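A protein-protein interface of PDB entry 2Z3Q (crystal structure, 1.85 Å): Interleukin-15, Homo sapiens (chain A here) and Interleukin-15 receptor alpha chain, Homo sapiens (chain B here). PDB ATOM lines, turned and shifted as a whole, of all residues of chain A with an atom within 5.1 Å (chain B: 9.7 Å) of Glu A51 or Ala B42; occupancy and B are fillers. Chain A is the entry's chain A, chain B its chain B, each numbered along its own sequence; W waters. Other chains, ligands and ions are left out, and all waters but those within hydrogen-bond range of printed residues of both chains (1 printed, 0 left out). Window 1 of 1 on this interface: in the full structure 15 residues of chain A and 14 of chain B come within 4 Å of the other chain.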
ATOM      1  N   THR A  29      34.240 -14.368  23.444  1.00  0.00           N
ATOM      2  CA  THR A  29      34.900 -14.833  24.618  1.00  0.00           C
ATOM      3  C   THR A  29      34.028 -15.990  24.976  1.00  0.00           C
ATOM      4  O   THR A  29      32.817 -15.975  24.730  1.00  0.00           O
ATOM      5  CB  THR A  29      34.979 -13.737  25.689  1.00  0.00           C
ATOM      6  OG1 THR A  29      33.692 -13.183  25.889  1.00  0.00           O
ATOM      7  CG2 THR A  29      35.867 -12.634  25.196  1.00  0.00           C
ATOM      8  N   LEU A  30      34.669 -17.031  25.465  1.00  0.00           N
ATOM      9  CA  LEU A  30      34.024 -18.304  25.713  1.00  0.00           C
ATOM     10  C   LEU A  30      34.404 -18.764  27.109  1.00  0.00           C
ATOM     11  O   LEU A  30      35.496 -18.513  27.551  1.00  0.00           O
ATOM     12  CB  LEU A  30      34.585 -19.349  24.728  1.00  0.00           C
ATOM     13  CG  LEU A  30      34.339 -18.998  23.256  1.00  0.00           C
ATOM     14  CD1 LEU A  30      35.006 -20.013  22.363  1.00  0.00           C
ATOM     15  CD2 LEU A  30      32.853 -19.017  23.003  1.00  0.00           C
ATOM     16  N   TYR A  31      33.492 -19.459  27.763  1.00  0.00           N
ATOM     17  CA  TYR A  31      33.702 -20.026  29.120  1.00  0.00           C
ATOM     18  C   TYR A  31      34.807 -21.087  29.052  1.00  0.00           C
ATOM     19  O   TYR A  31      34.714 -22.093  28.312  1.00  0.00           O
ATOM     20  CB  TYR A  31      32.400 -20.610  29.677  1.00  0.00           C
ATOM     21  CG  TYR A  31      31.246 -19.587  29.820  1.00  0.00           C
ATOM     22  CD1 TYR A  31      31.363 -18.522  30.705  1.00  0.00           C
ATOM     23  CD2 TYR A  31      30.059 -19.727  29.136  1.00  0.00           C
ATOM     24  CE1 TYR A  31      30.367 -17.606  30.860  1.00  0.00           C
ATOM     25  CE2 TYR A  31      29.027 -18.806  29.297  1.00  0.00           C
ATOM     26  CZ  TYR A  31      29.179 -17.770  30.142  1.00  0.00           C
ATOM     27  OH  TYR A  31      28.207 -16.840  30.302  1.00  0.00           O
ATOM     28  N   CYS A  47      31.152 -28.380  29.030  1.00  0.00           N
ATOM     29  CA  CYS A  47      31.226 -26.919  28.756  1.00  0.00           C
ATOM     30  C   CYS A  47      32.028 -26.557  27.544  1.00  0.00           C
ATOM     31  O   CYS A  47      31.579 -25.744  26.753  1.00  0.00           O
ATOM     32  CB  CYS A  47      31.785 -26.148  29.964  1.00  0.00           C
ATOM     33  SG  CYS A  47      30.797 -26.358  31.466  1.00  0.00           S
ATOM     34  N   PHE A  48      33.257 -27.075  27.450  1.00  0.00           N
ATOM     35  CA  PHE A  48      34.045 -26.931  26.228  1.00  0.00           C
ATOM     36  C   PHE A  48      33.280 -27.313  24.959  1.00  0.00           C
ATOM     37  O   PHE A  48      33.387 -26.574  23.964  1.00  0.00           O
ATOM     38  CB  PHE A  48      35.342 -27.733  26.277  1.00  0.00           C
ATOM     39  CG  PHE A  48      36.401 -27.102  27.084  1.00  0.00           C
ATOM     40  CD1 PHE A  48      37.103 -25.973  26.615  1.00  0.00           C
ATOM     41  CD2 PHE A  48      36.683 -27.610  28.339  1.00  0.00           C
ATOM     42  CE1 PHE A  48      38.088 -25.373  27.431  1.00  0.00           C
ATOM     43  CE2 PHE A  48      37.657 -27.058  29.127  1.00  0.00           C
ATOM     44  CZ  PHE A  48      38.361 -25.915  28.654  1.00  0.00           C
ATOM     45  N   LEU A  49      32.548 -28.454  24.978  1.00  0.00           N
ATOM     46  CA  LEU A  49      31.779 -28.914  23.801  1.00  0.00           C
ATOM     47  C   LEU A  49      30.656 -27.938  23.401  1.00  0.00           C
ATOM     48  O   LEU A  49      30.459 -27.633  22.212  1.00  0.00           O
ATOM     49  CB  LEU A  49      31.181 -30.322  24.025  1.00  0.00           C
ATOM     50  CG  LEU A  49      32.266 -31.421  24.122  1.00  0.00           C
ATOM     51  CD1 LEU A  49      31.670 -32.703  24.663  1.00  0.00           C
ATOM     52  CD2 LEU A  49      32.873 -31.621  22.716  1.00  0.00           C
ATOM     53  N   LEU A  50      29.911 -27.453  24.397  1.00  0.00           N
ATOM     54  CA  LEU A  50      28.936 -26.396  24.204  1.00  0.00           C
ATOM     55  C   LEU A  50      29.505 -25.154  23.578  1.00  0.00           C
ATOM     56  O   LEU A  50      28.927 -24.620  22.625  1.00  0.00           O
ATOM     57  CB  LEU A  50      28.202 -26.020  25.505  1.00  0.00           C
ATOM     58  CG  LEU A  50      27.148 -26.995  25.922  1.00  0.00           C
ATOM     59  CD1 LEU A  50      26.747 -26.620  27.344  1.00  0.00           C
ATOM     60  CD2 LEU A  50      25.908 -26.995  24.979  1.00  0.00           C
ATOM     61  N   GLU A  51      30.595 -24.675  24.128  1.00  0.00           N
ATOM     62  CA  GLU A  51      31.083 -23.402  23.713  1.00  0.00           C
ATOM     63  C   GLU A  51      31.716 -23.515  22.381  1.00  0.00           C
ATOM     64  O   GLU A  51      31.796 -22.531  21.655  1.00  0.00           O
ATOM     65  CB  GLU A  51      32.059 -22.856  24.739  1.00  0.00           C
ATOM     66  CG  GLU A  51      31.349 -22.390  26.043  1.00  0.00           C
ATOM     67  CD  GLU A  51      30.707 -21.032  25.851  1.00  0.00           C
ATOM     68  OE1 GLU A  51      31.392 -20.029  26.146  1.00  0.00           O
ATOM     69  OE2 GLU A  51      29.533 -20.956  25.412  1.00  0.00           O
ATOM     70  N   LEU A  52      32.229 -24.704  22.074  1.00  0.00           N
ATOM     71  CA  LEU A  52      32.740 -24.966  20.704  1.00  0.00           C
ATOM     72  C   LEU A  52      31.683 -24.690  19.622  1.00  0.00           C
ATOM     73  O   LEU A  52      32.026 -24.238  18.528  1.00  0.00           O
ATOM     74  CB  LEU A  52      33.312 -26.403  20.568  1.00  0.00           C
ATOM     75  CG  LEU A  52      34.216 -26.661  19.372  1.00  0.00           C
ATOM     76  CD1 LEU A  52      35.449 -25.869  19.284  1.00  0.00           C
ATOM     77  CD2 LEU A  52      34.589 -28.104  19.383  1.00  0.00           C
ATOM     78  N   GLN A  53      30.420 -24.965  19.898  1.00  0.00           N
ATOM     79  CA  GLN A  53      29.383 -24.660  18.951  1.00  0.00           C
ATOM     80  C   GLN A  53      29.230 -23.156  18.614  1.00  0.00           C
ATOM     81  O   GLN A  53      28.661 -22.777  17.552  1.00  0.00           O
ATOM     82  CB  GLN A  53      28.040 -25.143  19.484  1.00  0.00           C
ATOM     83  CG  GLN A  53      28.053 -26.597  19.940  1.00  0.00           C
ATOM     84  CD  GLN A  53      26.651 -27.058  20.326  1.00  0.00           C
ATOM     85  OE1 GLN A  53      25.906 -27.563  19.479  1.00  0.00           O
ATOM     86  NE2 GLN A  53      26.254 -26.811  21.571  1.00  0.00           N
ATOM     87  N   VAL A  54      29.646 -22.303  19.542  1.00  0.00           N
ATOM     88  CA  VAL A  54      29.586 -20.857  19.344  1.00  0.00           C
ATOM     89  C   VAL A  54      30.605 -20.504  18.296  1.00  0.00           C
ATOM     90  O   VAL A  54      30.351 -19.657  17.460  1.00  0.00           O
ATOM     91  CB  VAL A  54      29.913 -20.120  20.682  1.00  0.00           C
ATOM     92  CG1 VAL A  54      29.958 -18.607  20.485  1.00  0.00           C
ATOM     93  CG2 VAL A  54      28.845 -20.459  21.751  1.00  0.00           C
ATOM     94  N   ILE A  55      31.814 -21.078  18.406  1.00  0.00           N
ATOM     95  CA  ILE A  55      32.818 -20.827  17.384  1.00  0.00           C
ATOM     96  C   ILE A  55      32.319 -21.168  15.987  1.00  0.00           C
ATOM     97  O   ILE A  55      32.556 -20.408  15.009  1.00  0.00           O
ATOM     98  CB  ILE A  55      34.034 -21.654  17.654  1.00  0.00           C
ATOM     99  CG1 ILE A  55      34.738 -21.095  18.877  1.00  0.00           C
ATOM    100  CG2 ILE A  55      35.019 -21.496  16.509  1.00  0.00           C
ATOM    101  CD1 ILE A  55      35.964 -21.948  19.208  1.00  0.00           C
ATOM    102  N   CYS A  93      28.820 -23.955  33.804  1.00  0.00           N
ATOM    103  CA  CYS A  93      29.666 -23.356  32.741  1.00  0.00           C
ATOM    104  C   CYS A  93      29.787 -21.834  32.872  1.00  0.00           C
ATOM    105  O   CYS A  93      30.834 -21.267  32.566  1.00  0.00           O
ATOM    106  CB  CYS A  93      29.100 -23.708  31.351  1.00  0.00           C
ATOM    107  SG  CYS A  93      28.948 -25.511  31.016  1.00  0.00           S
ATOM    108  N   GLU A  94      28.705 -21.199  33.305  1.00  0.00           N
ATOM    109  CA  GLU A  94      28.543 -19.738  33.275  1.00  0.00           C
ATOM    110  C   GLU A  94      29.238 -19.114  34.487  1.00  0.00           C
ATOM    111  O   GLU A  94      29.332 -17.883  34.573  1.00  0.00           O
ATOM    112  CB  GLU A  94      27.064 -19.315  33.227  1.00  0.00           C
ATOM    113  CG  GLU A  94      26.379 -19.684  31.922  1.00  0.00           C
ATOM    114  CD  GLU A  94      25.921 -21.135  31.938  1.00  0.00           C
ATOM    115  OE1 GLU A  94      25.942 -21.777  33.024  1.00  0.00           O
ATOM    116  OE2 GLU A  94      25.538 -21.622  30.880  1.00  0.00           O
ATOM    117  N   PHE A 104      40.995 -20.395  24.952  1.00  0.00           N
ATOM    118  CA  PHE A 104      39.920 -21.383  25.039  1.00  0.00           C
ATOM    119  C   PHE A 104      40.372 -22.690  24.418  1.00  0.00           C
ATOM    120  O   PHE A 104      40.263 -23.759  25.025  1.00  0.00           O
ATOM    121  CB  PHE A 104      38.640 -20.886  24.314  1.00  0.00           C
ATOM    122  CG  PHE A 104      37.561 -21.942  24.189  1.00  0.00           C
ATOM    123  CD1 PHE A 104      36.674 -22.198  25.262  1.00  0.00           C
ATOM    124  CD2 PHE A 104      37.393 -22.660  22.981  1.00  0.00           C
ATOM    125  CE1 PHE A 104      35.675 -23.203  25.149  1.00  0.00           C
ATOM    126  CE2 PHE A 104      36.412 -23.632  22.812  1.00  0.00           C
ATOM    127  CZ  PHE A 104      35.507 -23.905  23.867  1.00  0.00           C
ATOM    128  N   ARG B  31      26.570  -7.249  18.902  1.00  0.00           N
ATOM    129  CA  ARG B  31      26.454  -8.229  19.962  1.00  0.00           C
ATOM    130  C   ARG B  31      25.619  -7.695  21.051  1.00  0.00           C
ATOM    131  O   ARG B  31      25.929  -6.619  21.548  1.00  0.00           O
ATOM    132  CB  ARG B  31      27.813  -8.478  20.608  1.00  0.00           C
ATOM    133  CG  ARG B  31      28.566  -9.546  19.956  1.00  0.00           C
ATOM    134  CD  ARG B  31      29.778  -9.940  20.778  1.00  0.00           C
ATOM    135  NE  ARG B  31      30.592 -10.609  19.804  1.00  0.00           N
ATOM    136  CZ  ARG B  31      30.478 -11.897  19.487  1.00  0.00           C
ATOM    137  NH1 ARG B  31      31.281 -12.397  18.564  1.00  0.00           N
ATOM    138  NH2 ARG B  31      29.638 -12.684  20.132  1.00  0.00           N
ATOM    139  N   CYS B  34      24.359  -9.510  28.036  1.00  0.00           N
ATOM    140  CA  CYS B  34      23.406  -9.840  29.097  1.00  0.00           C
ATOM    141  C   CYS B  34      23.473  -8.779  30.152  1.00  0.00           C
ATOM    142  O   CYS B  34      24.548  -8.230  30.433  1.00  0.00           O
ATOM    143  CB  CYS B  34      23.646 -11.232  29.700  1.00  0.00           C
ATOM    144  SG  CYS B  34      23.419 -12.543  28.477  1.00  0.00           S
ATOM    145  N   LYS B  39      23.920 -14.011  32.662  1.00  0.00           N
ATOM    146  CA  LYS B  39      25.099 -14.514  31.945  1.00  0.00           C
ATOM    147  C   LYS B  39      24.627 -15.166  30.650  1.00  0.00           C
ATOM    148  O   LYS B  39      23.559 -15.759  30.635  1.00  0.00           O
ATOM    149  CB  LYS B  39      25.782 -15.592  32.810  1.00  0.00           C
ATOM    150  CG  LYS B  39      26.517 -15.053  34.048  1.00  0.00           C
ATOM    151  CD  LYS B  39      27.746 -14.274  33.642  1.00  0.00           C
ATOM    152  CE  LYS B  39      28.479 -13.792  34.863  1.00  0.00           C
ATOM    153  NZ  LYS B  39      29.025 -12.432  34.512  1.00  0.00           N
ATOM    154  N   ARG B  40      25.394 -15.007  29.569  1.00  0.00           N
ATOM    155  CA  ARG B  40      25.142 -15.750  28.330  1.00  0.00           C
ATOM    156  C   ARG B  40      25.139 -17.222  28.638  1.00  0.00           C
ATOM    157  O   ARG B  40      26.060 -17.742  29.299  1.00  0.00           O
ATOM    158  CB  ARG B  40      26.224 -15.430  27.291  1.00  0.00           C
ATOM    159  CG  ARG B  40      26.214 -16.299  26.116  1.00  0.00           C
ATOM    160  CD  ARG B  40      27.263 -15.808  25.119  1.00  0.00           C
ATOM    161  NE  ARG B  40      28.589 -16.106  25.659  1.00  0.00           N
ATOM    162  CZ  ARG B  40      29.128 -17.335  25.696  1.00  0.00           C
ATOM    163  NH1 ARG B  40      28.484 -18.396  25.183  1.00  0.00           N
ATOM    164  NH2 ARG B  40      30.328 -17.505  26.216  1.00  0.00           N
ATOM    165  N   LYS B  41      24.097 -17.910  28.192  1.00  0.00           N
ATOM    166  CA  LYS B  41      24.030 -19.345  28.415  1.00  0.00           C
ATOM    167  C   LYS B  41      25.081 -20.042  27.560  1.00  0.00           C
ATOM    168  O   LYS B  41      25.222 -19.745  26.373  1.00  0.00           O
ATOM    169  CB  LYS B  41      22.661 -19.901  28.040  1.00  0.00           C
ATOM    170  CG  LYS B  41      22.589 -21.374  28.288  1.00  0.00           C
ATOM    171  CD  LYS B  41      21.214 -21.834  28.147  1.00  0.00           C
ATOM    172  CE  LYS B  41      21.121 -23.321  28.437  1.00  0.00           C
ATOM    173  NZ  LYS B  41      19.719 -23.711  28.122  1.00  0.00           N
ATOM    174  N   ALA B  42      25.792 -20.976  28.151  1.00  0.00           N
ATOM    175  CA  ALA B  42      26.827 -21.642  27.430  1.00  0.00           C
ATOM    176  C   ALA B  42      26.232 -22.328  26.206  1.00  0.00           C
ATOM    177  O   ALA B  42      25.177 -22.966  26.289  1.00  0.00           O
ATOM    178  CB  ALA B  42      27.515 -22.683  28.349  1.00  0.00           C
ATOM    179  N   GLY B  43      26.944 -22.233  25.088  1.00  0.00           N
ATOM    180  CA  GLY B  43      26.445 -22.850  23.875  1.00  0.00           C
ATOM    181  C   GLY B  43      25.646 -21.896  23.019  1.00  0.00           C
ATOM    182  O   GLY B  43      25.430 -22.191  21.850  1.00  0.00           O
ATOM    183  N   THR B  44      25.216 -20.766  23.583  1.00  0.00           N
ATOM    184  CA  THR B  44      24.406 -19.760  22.835  1.00  0.00           C
ATOM    185  C   THR B  44      25.307 -18.604  22.444  1.00  0.00           C
ATOM    186  O   THR B  44      26.350 -18.404  23.087  1.00  0.00           O
ATOM    187  CB  THR B  44      23.119 -19.250  23.586  1.00  0.00           C
ATOM    188  OG1 THR B  44      23.444 -18.412  24.687  1.00  0.00           O
ATOM    189  CG2 THR B  44      22.259 -20.413  24.086  1.00  0.00           C
ATOM    190  N   SER B  45      24.962 -17.915  21.344  1.00  0.00           N
ATOM    191  CA  SER B  45      25.804 -16.865  20.798  1.00  0.00           C
ATOM    192  C   SER B  45      25.103 -15.516  20.916  1.00  0.00           C
ATOM    193  O   SER B  45      23.894 -15.396  20.621  1.00  0.00           O
ATOM    194  CB  SER B  45      26.102 -17.186  19.332  1.00  0.00           C
ATOM    195  OG  SER B  45      26.661 -16.031  18.699  1.00  0.00           O
ATOM    196  N   SER B  46      25.840 -14.473  21.298  1.00  0.00           N
ATOM    197  CA  SER B  46      25.240 -13.109  21.344  1.00  0.00           C
ATOM    198  C   SER B  46      25.383 -12.262  19.997  1.00  0.00           C
ATOM    199  O   SER B  46      24.908 -11.146  19.907  1.00  0.00           O
ATOM    200  CB  SER B  46      25.892 -12.379  22.477  1.00  0.00           C
ATOM    201  OG  SER B  46      27.263 -12.231  22.162  1.00  0.00           O
ATOM    202  N   SER B  65      21.225 -16.716  18.917  1.00  0.00           N
ATOM    203  CA  SER B  65      20.717 -17.876  19.650  1.00  0.00           C
ATOM    204  C   SER B  65      20.771 -17.584  21.133  1.00  0.00           C
ATOM    205  O   SER B  65      20.299 -18.356  21.920  1.00  0.00           O
ATOM    206  CB  SER B  65      21.526 -19.134  19.352  1.00  0.00           C
ATOM    207  OG  SER B  65      22.900 -18.896  19.594  1.00  0.00           O
ATOM    208  N   LEU B  66      21.355 -16.451  21.500  1.00  0.00           N
ATOM    209  CA  LEU B  66      21.482 -15.991  22.882  1.00  0.00           C
ATOM    210  C   LEU B  66      20.294 -16.228  23.830  1.00  0.00           C
ATOM    211  O   LEU B  66      19.148 -15.854  23.534  1.00  0.00           O
ATOM    212  CB  LEU B  66      21.777 -14.501  22.890  1.00  0.00           C
ATOM    213  CG  LEU B  66      21.977 -13.896  24.280  1.00  0.00           C
ATOM    214  CD1 LEU B  66      23.219 -14.491  24.982  1.00  0.00           C
ATOM    215  CD2 LEU B  66      22.080 -12.405  24.137  1.00  0.00           C
ATOM    216  N   LYS B  67      20.591 -16.886  24.956  1.00  0.00           N
ATOM    217  CA  LYS B  67      19.713 -16.911  26.113  1.00  0.00           C
ATOM    218  C   LYS B  67      20.549 -16.351  27.264  1.00  0.00           C
ATOM    219  O   LYS B  67      21.701 -16.784  27.500  1.00  0.00           O
ATOM    220  CB  LYS B  67      19.197 -18.347  26.415  1.00  0.00           C
ATOM    221  CG  LYS B  67      18.135 -18.436  27.542  1.00  0.00           C
ATOM    222  CD  LYS B  67      16.708 -18.167  27.000  1.00  0.00           C
ATOM    223  CE  LYS B  67      15.655 -17.862  28.096  1.00  0.00           C
ATOM    224  NZ  LYS B  67      15.745 -18.849  29.203  1.00  0.00           N
ATOM    225  N   CYS B  68      20.009 -15.360  27.955  1.00  0.00           N
ATOM    226  CA  CYS B  68      20.649 -14.828  29.143  1.00  0.00           C
ATOM    227  C   CYS B  68      19.995 -15.493  30.335  1.00  0.00           C
ATOM    228  O   CYS B  68      18.784 -15.498  30.441  1.00  0.00           O
ATOM    229  CB  CYS B  68      20.498 -13.300  29.212  1.00  0.00           C
ATOM    230  SG  CYS B  68      21.432 -12.489  27.911  1.00  0.00           S
ATOM    231  N   ILE B  69      20.776 -16.123  31.204  1.00  0.00           N
ATOM    232  CA  ILE B  69      20.164 -16.849  32.328  1.00  0.00           C
ATOM    233  C   ILE B  69      20.711 -16.199  33.569  1.00  0.00           C
ATOM    234  O   ILE B  69      21.716 -15.536  33.481  1.00  0.00           O
ATOM    235  CB  ILE B  69      20.505 -18.342  32.296  1.00  0.00           C
ATOM    236  CG1 ILE B  69      22.042 -18.521  32.341  1.00  0.00           C
ATOM    237  CG2 ILE B  69      19.897 -18.987  31.023  1.00  0.00           C
ATOM    238  CD1 ILE B  69      22.532 -19.922  32.513  1.00  0.00           C
ATOM    239  N   ARG B  70      20.032 -16.337  34.699  1.00  0.00           N
ATOM    240  CA  ARG B  70      20.509 -15.838  35.973  1.00  0.00           C
ATOM    241  C   ARG B  70      21.915 -16.341  36.266  1.00  0.00           C
ATOM    242  O   ARG B  70      22.203 -17.518  36.108  1.00  0.00           O
ATOM    243  CB  ARG B  70      19.569 -16.321  37.085  1.00  0.00           C
ATOM    244  CG  ARG B  70      18.863 -15.257  37.827  1.00  0.00           C
ATOM    245  CD  ARG B  70      19.720 -14.626  38.932  1.00  0.00           C
ATOM    246  NE  ARG B  70      19.987 -13.221  38.628  1.00  0.00           N
ATOM    247  CZ  ARG B  70      20.302 -12.284  39.521  1.00  0.00           C
ATOM    248  NH1 ARG B  70      20.406 -12.575  40.812  1.00  0.00           N
ATOM    249  NH2 ARG B  70      20.503 -11.038  39.115  1.00  0.00           N
ATOM    250  N   PRO B  72      24.768 -18.068  37.833  1.00  0.00           N
ATOM    251  CA  PRO B  72      24.711 -19.168  38.797  1.00  0.00           C
ATOM    252  C   PRO B  72      25.389 -18.824  40.103  1.00  0.00           C
ATOM    253  O   PRO B  72      25.038 -19.393  41.125  1.00  0.00           O
ATOM    254  CB  PRO B  72      25.453 -20.312  38.106  1.00  0.00           C
ATOM    255  CG  PRO B  72      25.599 -19.894  36.688  1.00  0.00           C
ATOM    256  CD  PRO B  72      25.505 -18.437  36.616  1.00  0.00           C
HETATM  257  O   HOH W   1      30.681 -14.650  23.413  1.00  0.00           O
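The guanidinium group (NH2) of Arg B40 is in hydrogen-bond range of the backbone carbonyl oxygen (O) of Thr A29 (3.3 Å).
OH of Tyr A31 is in hydrogen-bond range of O of Arg B40 (2.5 Å).
The side-chain carboxylate (OE1) of Glu A51 lies within salt-bridge range of the guanidinium group (NH2) of Arg B40, 2.7 Å away.
N of Gly B43 is in hydrogen-bond range of OE2 of Glu A51, 2.9 Å away.
The backbone NH of Ala B42 lies within hydrogen-bond range of the side-chain carboxylate of Glu A94 (2.8 Å).
The backbone NH (N) of Lys B39 lies within hydrogen-bond range of the backbone carbonyl oxygen (O) of Ile B69 (2.8 Å).
O of Thr B44 is in hydrogen-bond range of NH1 of Arg B40 (3.0 Å).
The backbone carbonyl oxygen (O) of Lys B41 lies within hydrogen-bond range of the side-chain hydroxyl (OG1) of Thr B44 (2.8 Å).
The backbone carbonyl oxygen (O) of Lys B67 is in hydrogen-bond range of the backbone NH (N) of Lys B41 (2.7 Å).
The side-chain hydroxyl (OG1) of Thr B44 lies within hydrogen-bond range of the backbone NH (N) of Lys B67, at 3.2 Å.
SG of Cys B34 is disulfide-bonded to SG of Cys B68.
CA of Leu A30 touches NH2 of Arg B40 (3.8 Å).
Ala B42 touches Tyr A31.
O of Leu A50 touches CA of Gly B43, at 3.3 Å.
Val A54 touches Gly B43.
Val A54 touches Thr B44 (CG2 to O, 3.5 Å).
Cys A93 touches Ala B42 (CB to CB, 3.5 Å).
Glu A94 touches Lys B39.
CG of Glu A94 touches O of Arg B40, 3.3 Å away.
Lys B41 touches Glu A94.
Ile B69 touches Glu A94.
Of chain B, only Arg B40 (3.8 Å) comes within 4 Å of Leu A30.
Of chain B, only Arg B40, Ala B42 and Gly B43 come within 4 Å of Glu A51.
Of the printed residues of chain A, Lys B41 touches Glu A94 (3.7 Å).
Ala B42 touches four residues of chain A.
Of the printed residues of chain A, Gly B43 touches Leu A50, Glu A51 and Val A54.
Printed residues of chain A within 4 Å of Thr B44: Val A54.
Ser B46 touches none of the printed residues of chain A.
Ser B65 touches none of the printed residues of chain A.
The nearest residue of chain A that does not touch Ala B42 is Leu A50 (4.1 Å).
The nearest printed residue of chain A that does not touch Lys B41 is Tyr A31 (4.5 Å).
Hydrophobic or aromatic side chains of chain A within 4 Å of the printed part of chain B: Tyr A31, Leu A50 and Val A54.
Along chain A the printed residues that touch a printed residue of chain B span positions 29 to 94.
Printed residues of chain B that touch a printed residue of chain A: Lys B39, Arg B40, Lys B41, Ala B42, Gly B43, Thr B44, Ile B69 and Pro B72.
Hydrophobic or aromatic side chains of chain B that line the printed part of chain A: Ala B42, Ile B69 and Pro B72.
Among the printed residues, 18 pairs touch across the chains.
Water W1 lies within hydrogen-bond range of O of Thr A29 (2.8 Å) and NE of Arg B40 (3.4 Å).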
